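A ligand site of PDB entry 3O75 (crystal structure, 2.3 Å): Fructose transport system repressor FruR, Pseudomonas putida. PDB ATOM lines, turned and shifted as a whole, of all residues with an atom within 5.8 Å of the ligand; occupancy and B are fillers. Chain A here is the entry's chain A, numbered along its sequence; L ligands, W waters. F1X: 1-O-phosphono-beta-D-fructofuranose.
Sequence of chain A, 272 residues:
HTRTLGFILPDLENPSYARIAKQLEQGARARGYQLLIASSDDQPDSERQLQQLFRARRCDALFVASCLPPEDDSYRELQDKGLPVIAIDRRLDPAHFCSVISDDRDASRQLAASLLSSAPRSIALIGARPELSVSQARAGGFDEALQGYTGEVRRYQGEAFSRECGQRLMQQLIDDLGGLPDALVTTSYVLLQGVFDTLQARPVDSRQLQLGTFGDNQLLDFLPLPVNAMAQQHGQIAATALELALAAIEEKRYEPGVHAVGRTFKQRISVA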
ATOM      1  N   PRO A  10      14.869  18.436  10.571  1.00  0.00           N
ATOM      2  CA  PRO A  10      13.432  18.596  10.323  1.00  0.00           C
ATOM      3  C   PRO A  10      12.894  20.021  10.489  1.00  0.00           C
ATOM      4  O   PRO A  10      11.997  20.406   9.752  1.00  0.00           O
ATOM      5  CB  PRO A  10      12.791  17.681  11.381  1.00  0.00           C
ATOM      6  CG  PRO A  10      13.900  16.846  11.925  1.00  0.00           C
ATOM      7  CD  PRO A  10      15.127  17.676  11.813  1.00  0.00           C
ATOM      8  N   ASN A  14      12.892  24.628  15.633  1.00  0.00           N
ATOM      9  CA  ASN A  14      12.990  23.812  16.839  1.00  0.00           C
ATOM     10  C   ASN A  14      14.364  24.040  17.439  1.00  0.00           C
ATOM     11  O   ASN A  14      15.375  23.593  16.886  1.00  0.00           O
ATOM     12  CB  ASN A  14      12.776  22.335  16.509  1.00  0.00           C
ATOM     13  CG  ASN A  14      12.666  21.460  17.761  1.00  0.00           C
ATOM     14  OD1 ASN A  14      13.465  21.592  18.687  1.00  0.00           O
ATOM     15  ND2 ASN A  14      11.689  20.578  17.780  1.00  0.00           N
ATOM     16  N   SER A  16      16.208  22.819  19.664  1.00  0.00           N
ATOM     17  CA  SER A  16      17.106  21.677  19.849  1.00  0.00           C
ATOM     18  C   SER A  16      17.919  21.368  18.594  1.00  0.00           C
ATOM     19  O   SER A  16      19.124  21.099  18.677  1.00  0.00           O
ATOM     20  CB  SER A  16      16.336  20.449  20.331  1.00  0.00           C
ATOM     21  OG  SER A  16      15.973  20.586  21.693  1.00  0.00           O
ATOM     22  N   TYR A  17      17.272  21.387  17.427  1.00  0.00           N
ATOM     23  CA  TYR A  17      18.000  21.172  16.184  1.00  0.00           C
ATOM     24  C   TYR A  17      18.970  22.308  15.890  1.00  0.00           C
ATOM     25  O   TYR A  17      20.113  22.062  15.487  1.00  0.00           O
ATOM     26  CB  TYR A  17      17.046  20.934  15.009  1.00  0.00           C
ATOM     27  CG  TYR A  17      16.346  19.597  15.093  1.00  0.00           C
ATOM     28  CD1 TYR A  17      14.986  19.515  15.386  1.00  0.00           C
ATOM     29  CD2 TYR A  17      17.044  18.411  14.907  1.00  0.00           C
ATOM     30  CE1 TYR A  17      14.353  18.294  15.475  1.00  0.00           C
ATOM     31  CE2 TYR A  17      16.423  17.188  14.989  1.00  0.00           C
ATOM     32  CZ  TYR A  17      15.073  17.133  15.270  1.00  0.00           C
ATOM     33  OH  TYR A  17      14.440  15.913  15.360  1.00  0.00           O
ATOM     34  N   ASP A  42      10.127  17.949   7.933  1.00  0.00           N
ATOM     35  CA  ASP A  42       9.547  16.652   8.269  1.00  0.00           C
ATOM     36  C   ASP A  42       8.673  16.077   7.154  1.00  0.00           C
ATOM     37  O   ASP A  42       7.685  15.389   7.429  1.00  0.00           O
ATOM     38  CB  ASP A  42       8.752  16.720   9.579  1.00  0.00           C
ATOM     39  CG  ASP A  42       9.461  16.025  10.731  1.00  0.00           C
ATOM     40  OD1 ASP A  42      10.310  15.153  10.473  1.00  0.00           O
ATOM     41  OD2 ASP A  42       9.174  16.358  11.901  1.00  0.00           O
ATOM     42  N   ASP A  89      19.114  11.830  16.466  1.00  0.00           N
ATOM     43  CA  ASP A  89      17.758  11.926  17.003  1.00  0.00           C
ATOM     44  C   ASP A  89      16.868  10.752  16.592  1.00  0.00           C
ATOM     45  O   ASP A  89      16.515   9.922  17.429  1.00  0.00           O
ATOM     46  CB  ASP A  89      17.108  13.261  16.636  1.00  0.00           C
ATOM     47  CG  ASP A  89      15.845  13.532  17.430  1.00  0.00           C
ATOM     48  OD1 ASP A  89      15.885  14.391  18.342  1.00  0.00           O
ATOM     49  OD2 ASP A  89      14.818  12.879  17.150  1.00  0.00           O
ATOM     50  N   ARG A  90      16.490  10.675  15.312  1.00  0.00           N
ATOM     51  CA  ARG A  90      15.738   9.516  14.814  1.00  0.00           C
ATOM     52  C   ARG A  90      16.674   8.436  14.292  1.00  0.00           C
ATOM     53  O   ARG A  90      17.434   8.664  13.353  1.00  0.00           O
ATOM     54  CB  ARG A  90      14.734   9.913  13.724  1.00  0.00           C
ATOM     55  CG  ARG A  90      13.611  10.840  14.194  1.00  0.00           C
ATOM     56  CD  ARG A  90      13.975  12.289  13.924  1.00  0.00           C
ATOM     57  NE  ARG A  90      12.858  13.193  14.167  1.00  0.00           N
ATOM     58  CZ  ARG A  90      11.988  13.584  13.239  1.00  0.00           C
ATOM     59  NH1 ARG A  90      12.089  13.112  12.000  1.00  0.00           N
ATOM     60  NH2 ARG A  90      11.018  14.425  13.551  1.00  0.00           N
ATOM     61  N   ASP A 104      14.789   7.825  24.734  1.00  0.00           N
ATOM     62  CA  ASP A 104      13.409   8.300  24.689  1.00  0.00           C
ATOM     63  C   ASP A 104      12.442   7.534  25.590  1.00  0.00           C
ATOM     64  O   ASP A 104      11.691   8.134  26.350  1.00  0.00           O
ATOM     65  CB  ASP A 104      12.902   8.300  23.234  1.00  0.00           C
ATOM     66  CG  ASP A 104      13.645   9.283  22.351  1.00  0.00           C
ATOM     67  OD1 ASP A 104      13.738  10.473  22.736  1.00  0.00           O
ATOM     68  OD2 ASP A 104      14.136   8.889  21.275  1.00  0.00           O
ATOM     69  N   LEU A 132       6.384   7.831  13.837  1.00  0.00           N
ATOM     70  CA  LEU A 132       7.832   7.933  14.026  1.00  0.00           C
ATOM     71  C   LEU A 132       8.348   7.062  15.170  1.00  0.00           C
ATOM     72  O   LEU A 132       7.694   6.915  16.199  1.00  0.00           O
ATOM     73  CB  LEU A 132       8.254   9.393  14.245  1.00  0.00           C
ATOM     74  CG  LEU A 132       8.408  10.246  12.992  1.00  0.00           C
ATOM     75  CD1 LEU A 132       8.846  11.651  13.369  1.00  0.00           C
ATOM     76  CD2 LEU A 132       9.399   9.604  12.027  1.00  0.00           C
ATOM     77  N   VAL A 134      10.759   7.643  17.242  1.00  0.00           N
ATOM     78  CA  VAL A 134      10.987   8.419  18.448  1.00  0.00           C
ATOM     79  C   VAL A 134       9.675   8.638  19.209  1.00  0.00           C
ATOM     80  O   VAL A 134       9.640   8.659  20.437  1.00  0.00           O
ATOM     81  CB  VAL A 134      11.669   9.764  18.137  1.00  0.00           C
ATOM     82  CG1 VAL A 134      10.714  10.705  17.419  1.00  0.00           C
ATOM     83  CG2 VAL A 134      12.179  10.397  19.406  1.00  0.00           C
ATOM     84  N   ARG A 138       8.394   7.228  23.016  1.00  0.00           N
ATOM     85  CA  ARG A 138       7.905   8.166  24.018  1.00  0.00           C
ATOM     86  C   ARG A 138       6.496   7.850  24.494  1.00  0.00           C
ATOM     87  O   ARG A 138       6.189   7.987  25.675  1.00  0.00           O
ATOM     88  CB  ARG A 138       8.000   9.609  23.500  1.00  0.00           C
ATOM     89  CG  ARG A 138       9.440  10.062  23.364  1.00  0.00           C
ATOM     90  CD  ARG A 138       9.572  11.413  22.661  1.00  0.00           C
ATOM     91  NE  ARG A 138      10.935  11.602  22.179  1.00  0.00           N
ATOM     92  CZ  ARG A 138      11.400  12.727  21.637  1.00  0.00           C
ATOM     93  NH1 ARG A 138      10.614  13.787  21.508  1.00  0.00           N
ATOM     94  NH2 ARG A 138      12.663  12.775  21.234  1.00  0.00           N
ATOM     95  N   PHE A 161       5.171  18.196  14.980  1.00  0.00           N
ATOM     96  CA  PHE A 161       5.831  18.778  16.140  1.00  0.00           C
ATOM     97  C   PHE A 161       5.897  20.292  15.990  1.00  0.00           C
ATOM     98  O   PHE A 161       6.920  20.839  15.566  1.00  0.00           O
ATOM     99  CB  PHE A 161       7.251  18.223  16.292  1.00  0.00           C
ATOM    100  CG  PHE A 161       7.300  16.774  16.701  1.00  0.00           C
ATOM    101  CD1 PHE A 161       7.539  15.780  15.755  1.00  0.00           C
ATOM    102  CD2 PHE A 161       7.109  16.399  18.017  1.00  0.00           C
ATOM    103  CE1 PHE A 161       7.592  14.448  16.130  1.00  0.00           C
ATOM    104  CE2 PHE A 161       7.162  15.067  18.392  1.00  0.00           C
ATOM    105  CZ  PHE A 161       7.399  14.086  17.450  1.00  0.00           C
ATOM    106  N   THR A 187       5.812  15.740  24.513  1.00  0.00           N
ATOM    107  CA  THR A 187       6.949  14.997  23.966  1.00  0.00           C
ATOM    108  C   THR A 187       7.983  15.862  23.238  1.00  0.00           C
ATOM    109  O   THR A 187       8.896  15.332  22.610  1.00  0.00           O
ATOM    110  CB  THR A 187       6.487  13.891  23.001  1.00  0.00           C
ATOM    111  OG1 THR A 187       5.835  14.490  21.877  1.00  0.00           O
ATOM    112  CG2 THR A 187       5.530  12.944  23.697  1.00  0.00           C
ATOM    113  N   SER A 188       7.822  17.177  23.325  1.00  0.00           N
ATOM    114  CA  SER A 188       8.780  18.111  22.739  1.00  0.00           C
ATOM    115  C   SER A 188       8.442  19.499  23.270  1.00  0.00           C
ATOM    116  O   SER A 188       7.269  19.802  23.477  1.00  0.00           O
ATOM    117  CB  SER A 188       8.669  18.094  21.209  1.00  0.00           C
ATOM    118  OG  SER A 188       9.484  19.105  20.628  1.00  0.00           O
ATOM    119  N   TYR A 189       9.458  20.330  23.504  1.00  0.00           N
ATOM    120  CA  TYR A 189       9.170  21.644  24.086  1.00  0.00           C
ATOM    121  C   TYR A 189       8.292  22.457  23.153  1.00  0.00           C
ATOM    122  O   TYR A 189       7.429  23.221  23.598  1.00  0.00           O
ATOM    123  CB  TYR A 189      10.427  22.432  24.425  1.00  0.00           C
ATOM    124  CG  TYR A 189      10.079  23.739  25.109  1.00  0.00           C
ATOM    125  CD1 TYR A 189       9.753  23.759  26.458  1.00  0.00           C
ATOM    126  CD2 TYR A 189      10.015  24.927  24.402  1.00  0.00           C
ATOM    127  CE1 TYR A 189       9.400  24.930  27.094  1.00  0.00           C
ATOM    128  CE2 TYR A 189       9.662  26.117  25.028  1.00  0.00           C
ATOM    129  CZ  TYR A 189       9.360  26.112  26.373  1.00  0.00           C
ATOM    130  OH  TYR A 189       9.015  27.271  27.028  1.00  0.00           O
ATOM    131  N   VAL A 190       8.523  22.292  21.852  1.00  0.00           N
ATOM    132  CA  VAL A 190       7.774  23.011  20.838  1.00  0.00           C
ATOM    133  C   VAL A 190       6.266  22.811  21.014  1.00  0.00           C
ATOM    134  O   VAL A 190       5.481  23.731  20.807  1.00  0.00           O
ATOM    135  CB  VAL A 190       8.220  22.604  19.425  1.00  0.00           C
ATOM    136  CG1 VAL A 190       7.122  22.864  18.424  1.00  0.00           C
ATOM    137  CG2 VAL A 190       9.488  23.346  19.046  1.00  0.00           C
ATOM    138  N   PHE A 214       9.371  16.961  27.415  1.00  0.00           N
ATOM    139  CA  PHE A 214      10.634  16.776  26.726  1.00  0.00           C
ATOM    140  C   PHE A 214      11.153  18.157  26.335  1.00  0.00           C
ATOM    141  O   PHE A 214      10.374  19.049  26.005  1.00  0.00           O
ATOM    142  CB  PHE A 214      10.454  15.898  25.491  1.00  0.00           C
ATOM    143  CG  PHE A 214      10.635  14.436  25.757  1.00  0.00           C
ATOM    144  CD1 PHE A 214       9.664  13.726  26.435  1.00  0.00           C
ATOM    145  CD2 PHE A 214      11.768  13.780  25.338  1.00  0.00           C
ATOM    146  CE1 PHE A 214       9.825  12.370  26.689  1.00  0.00           C
ATOM    147  CE2 PHE A 214      11.939  12.433  25.590  1.00  0.00           C
ATOM    148  CZ  PHE A 214      10.967  11.724  26.268  1.00  0.00           C
ATOM    149  N   GLY A 215      12.468  18.327  26.376  1.00  0.00           N
ATOM    150  CA  GLY A 215      13.064  19.627  26.112  1.00  0.00           C
ATOM    151  C   GLY A 215      13.121  20.478  27.364  1.00  0.00           C
ATOM    152  O   GLY A 215      12.705  20.057  28.440  1.00  0.00           O
ATOM    153  N   ASP A 216      13.635  21.693  27.202  1.00  0.00           N
ATOM    154  CA  ASP A 216      13.802  22.614  28.321  1.00  0.00           C
ATOM    155  C   ASP A 216      13.940  24.025  27.760  1.00  0.00           C
ATOM    156  O   ASP A 216      14.289  24.199  26.596  1.00  0.00           O
ATOM    157  CB  ASP A 216      15.040  22.242  29.138  1.00  0.00           C
ATOM    158  CG  ASP A 216      15.138  23.017  30.437  1.00  0.00           C
ATOM    159  OD1 ASP A 216      14.095  23.446  30.957  1.00  0.00           O
ATOM    160  OD2 ASP A 216      16.268  23.179  30.963  1.00  0.00           O
ATOM    161  N   MET A 230      12.960  17.008  30.607  1.00  0.00           N
ATOM    162  CA  MET A 230      14.011  16.100  30.178  1.00  0.00           C
ATOM    163  C   MET A 230      14.758  16.738  29.010  1.00  0.00           C
ATOM    164  O   MET A 230      14.325  16.655  27.855  1.00  0.00           O
ATOM    165  CB  MET A 230      13.412  14.761  29.740  1.00  0.00           C
ATOM    166  CG  MET A 230      12.989  13.858  30.881  1.00  0.00           C
ATOM    167  SD  MET A 230      14.381  13.045  31.703  1.00  0.00           S
ATOM    168  CE  MET A 230      13.493  11.989  32.848  1.00  0.00           C
ATOM    169  N   GLN A 232      17.825  17.343  26.316  1.00  0.00           N
ATOM    170  CA  GLN A 232      18.842  16.617  25.582  1.00  0.00           C
ATOM    171  C   GLN A 232      20.220  17.104  26.009  1.00  0.00           C
ATOM    172  O   GLN A 232      20.373  18.247  26.432  1.00  0.00           O
ATOM    173  CB  GLN A 232      18.716  16.868  24.076  1.00  0.00           C
ATOM    174  CG  GLN A 232      17.487  16.306  23.404  1.00  0.00           C
ATOM    175  CD  GLN A 232      17.528  16.527  21.898  1.00  0.00           C
ATOM    176  OE1 GLN A 232      18.492  16.146  21.231  1.00  0.00           O
ATOM    177  NE2 GLN A 232      16.492  17.154  21.360  1.00  0.00           N
ATOM    178  N   HIS A 234      22.642  18.168  24.035  1.00  0.00           N
ATOM    179  CA  HIS A 234      22.897  18.545  22.654  1.00  0.00           C
ATOM    180  C   HIS A 234      24.377  18.470  22.310  1.00  0.00           C
ATOM    181  O   HIS A 234      24.746  17.959  21.249  1.00  0.00           O
ATOM    182  CB  HIS A 234      22.395  19.962  22.376  1.00  0.00           C
ATOM    183  CG  HIS A 234      20.952  20.176  22.706  1.00  0.00           C
ATOM    184  ND1 HIS A 234      20.522  20.529  23.967  1.00  0.00           N
ATOM    185  CD2 HIS A 234      19.841  20.090  21.931  1.00  0.00           C
ATOM    186  CE1 HIS A 234      19.208  20.643  23.957  1.00  0.00           C
ATOM    187  NE2 HIS A 234      18.768  20.383  22.739  1.00  0.00           N
ATOM    188  N   ARG A 263      18.888  11.832  28.556  1.00  0.00           N
ATOM    189  CA  ARG A 263      18.441  13.200  28.762  1.00  0.00           C
ATOM    190  C   ARG A 263      18.671  13.640  30.215  1.00  0.00           C
ATOM    191  O   ARG A 263      18.673  12.820  31.124  1.00  0.00           O
ATOM    192  CB  ARG A 263      16.971  13.355  28.371  1.00  0.00           C
ATOM    193  CG  ARG A 263      16.692  13.138  26.875  1.00  0.00           C
ATOM    194  CD  ARG A 263      15.429  13.853  26.454  1.00  0.00           C
ATOM    195  NE  ARG A 263      15.257  13.874  25.005  1.00  0.00           N
ATOM    196  CZ  ARG A 263      14.647  14.855  24.331  1.00  0.00           C
ATOM    197  NH1 ARG A 263      14.171  15.909  24.982  1.00  0.00           N
ATOM    198  NH2 ARG A 263      14.530  14.799  23.014  1.00  0.00           N
HETATM  199  C1  F1X L   1      13.557  17.897  20.081  1.00  0.00           C
HETATM  200  O1  F1X L   1      12.903  18.815  20.937  1.00  0.00           O
HETATM  201  P1  F1X L   1      13.095  18.653  22.530  1.00  0.00           P
HETATM  202  C2  F1X L   1      12.534  16.891  19.565  1.00  0.00           C
HETATM  203  O2  F1X L   1      11.654  16.511  20.629  1.00  0.00           O
HETATM  204  C3  F1X L   1      13.239  15.671  18.997  1.00  0.00           C
HETATM  205  O3  F1X L   1      13.611  14.746  20.017  1.00  0.00           O
HETATM  206  C4  F1X L   1      12.180  15.140  18.066  1.00  0.00           C
HETATM  207  O4  F1X L   1      12.672  14.216  17.092  1.00  0.00           O
HETATM  208  C5  F1X L   1      11.756  16.454  17.446  1.00  0.00           C
HETATM  209  O5  F1X L   1      11.746  17.426  18.496  1.00  0.00           O
HETATM  210  C6  F1X L   1      10.432  16.312  16.747  1.00  0.00           C
HETATM  211  O6  F1X L   1      10.766  15.925  15.422  1.00  0.00           O
HETATM  212  O1P F1X L   1      12.593  17.274  22.833  1.00  0.00           O
HETATM  213  O2P F1X L   1      14.580  18.836  22.745  1.00  0.00           O
HETATM  214  O3P F1X L   1      12.238  19.752  23.108  1.00  0.00           O
HETATM  215  O   HOH W   1      16.234  13.269  21.182  1.00  0.00           O
HETATM  216  O   HOH W   2      10.645  18.589  14.805  1.00  0.00           O
HETATM  217  O   HOH W   3      16.158  19.303  24.845  1.00  0.00           O
HETATM  218  O   HOH W   4      12.169  21.862  21.292  1.00  0.00           O
HETATM  219  O   HOH W   5      13.890  22.116  23.945  1.00  0.00           O
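NH2 of Arg 90 lies within hydrogen-bond range of O6 of the ligand (2.4 Å). The side-chain hydroxyl (OG) of Ser 16 is in hydrogen-bond range of an oxygen (O2P) of the ligand, at 2.5 Å. O3 of the ligand lies within hydrogen-bond range of NH2 of Arg 138 (2.5 Å). An oxygen (O4) of the ligand lies within hydrogen-bond range of the side-chain carboxylate (OD2) of Asp 89 (2.5 Å). The backbone NH of Tyr 189 is in hydrogen-bond range of an oxygen (O3P) of the ligand (2.9 Å). NE2 of Gln 232 is in hydrogen-bond range of O2P of the ligand, at 2.9 Å. NH1 of Arg 263 lies within salt-bridge range of O1P of the ligand, 3.0 Å away. OH of Tyr 17 sits at hydrogen-bond distance from O4 of the ligand (3.0 Å). The side-chain amide nitrogen (ND2) of Asn 14 sits at hydrogen-bond distance from an oxygen (O5) of the ligand, at 3.2 Å. O2 of the ligand lies within hydrogen-bond range of OG of Ser 188, at 3.4 Å.
The guanidinium group (NE) of Arg 90 is in salt-bridge range of the side-chain carboxylate (OD2) of Asp 89 (3.6 Å). The guanidinium group (NH1) of Arg 90 lies within salt-bridge range of the side-chain carboxylate (OD1) of Asp 42 (3.1 Å). The backbone NH (N) of Ser 16 sits close to the side-chain amide oxygen (OD1) of Asn 14 (3.2 Å). The guanidinium group of Arg 138 is in salt-bridge range of the side-chain carboxylate of Asp 104, at 3.0 Å. The backbone NH (N) of Tyr 189 lies within hydrogen-bond range of the backbone carbonyl oxygen (O) of Phe 214, 3.0 Å away. O of Gln 232 lies within hydrogen-bond range of ND1 of His 234 (3.4 Å). O of Met 230 is in hydrogen-bond range of NH1 of Arg 263 (3.0 Å). O of Met 230 sits at hydrogen-bond distance from N of Gly 215 (2.9 Å).
Asp 42 touches the ligand. Phe 161 touches the ligand. Thr 187 touches the ligand (O to O2, 3.6 Å). Phe 214 touches the ligand. Gly 215 touches the ligand. Of the 23 residues printed, 15 come within 4 Å of the ligand.
Water W3 lies within hydrogen-bond range of an oxygen (O2P) of the ligand (2.7 Å), the backbone NH (N) of Gln 232 (3.0 Å) and the side-chain hydroxyl (OG) of Ser 16 (3.4 Å). Water W4 lies within hydrogen-bond range of O3P of the ligand and OD1 of Asn 14. Water W5 lies within hydrogen-bond range of an oxygen (O3P) of the ligand, the backbone NH (N) of Asp 216 and the side-chain hydroxyl (OG) of Ser 16. Water W1 lies within hydrogen-bond range of NH2 of Arg 263, OD1 of Asp 89 and O3 of the ligand.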
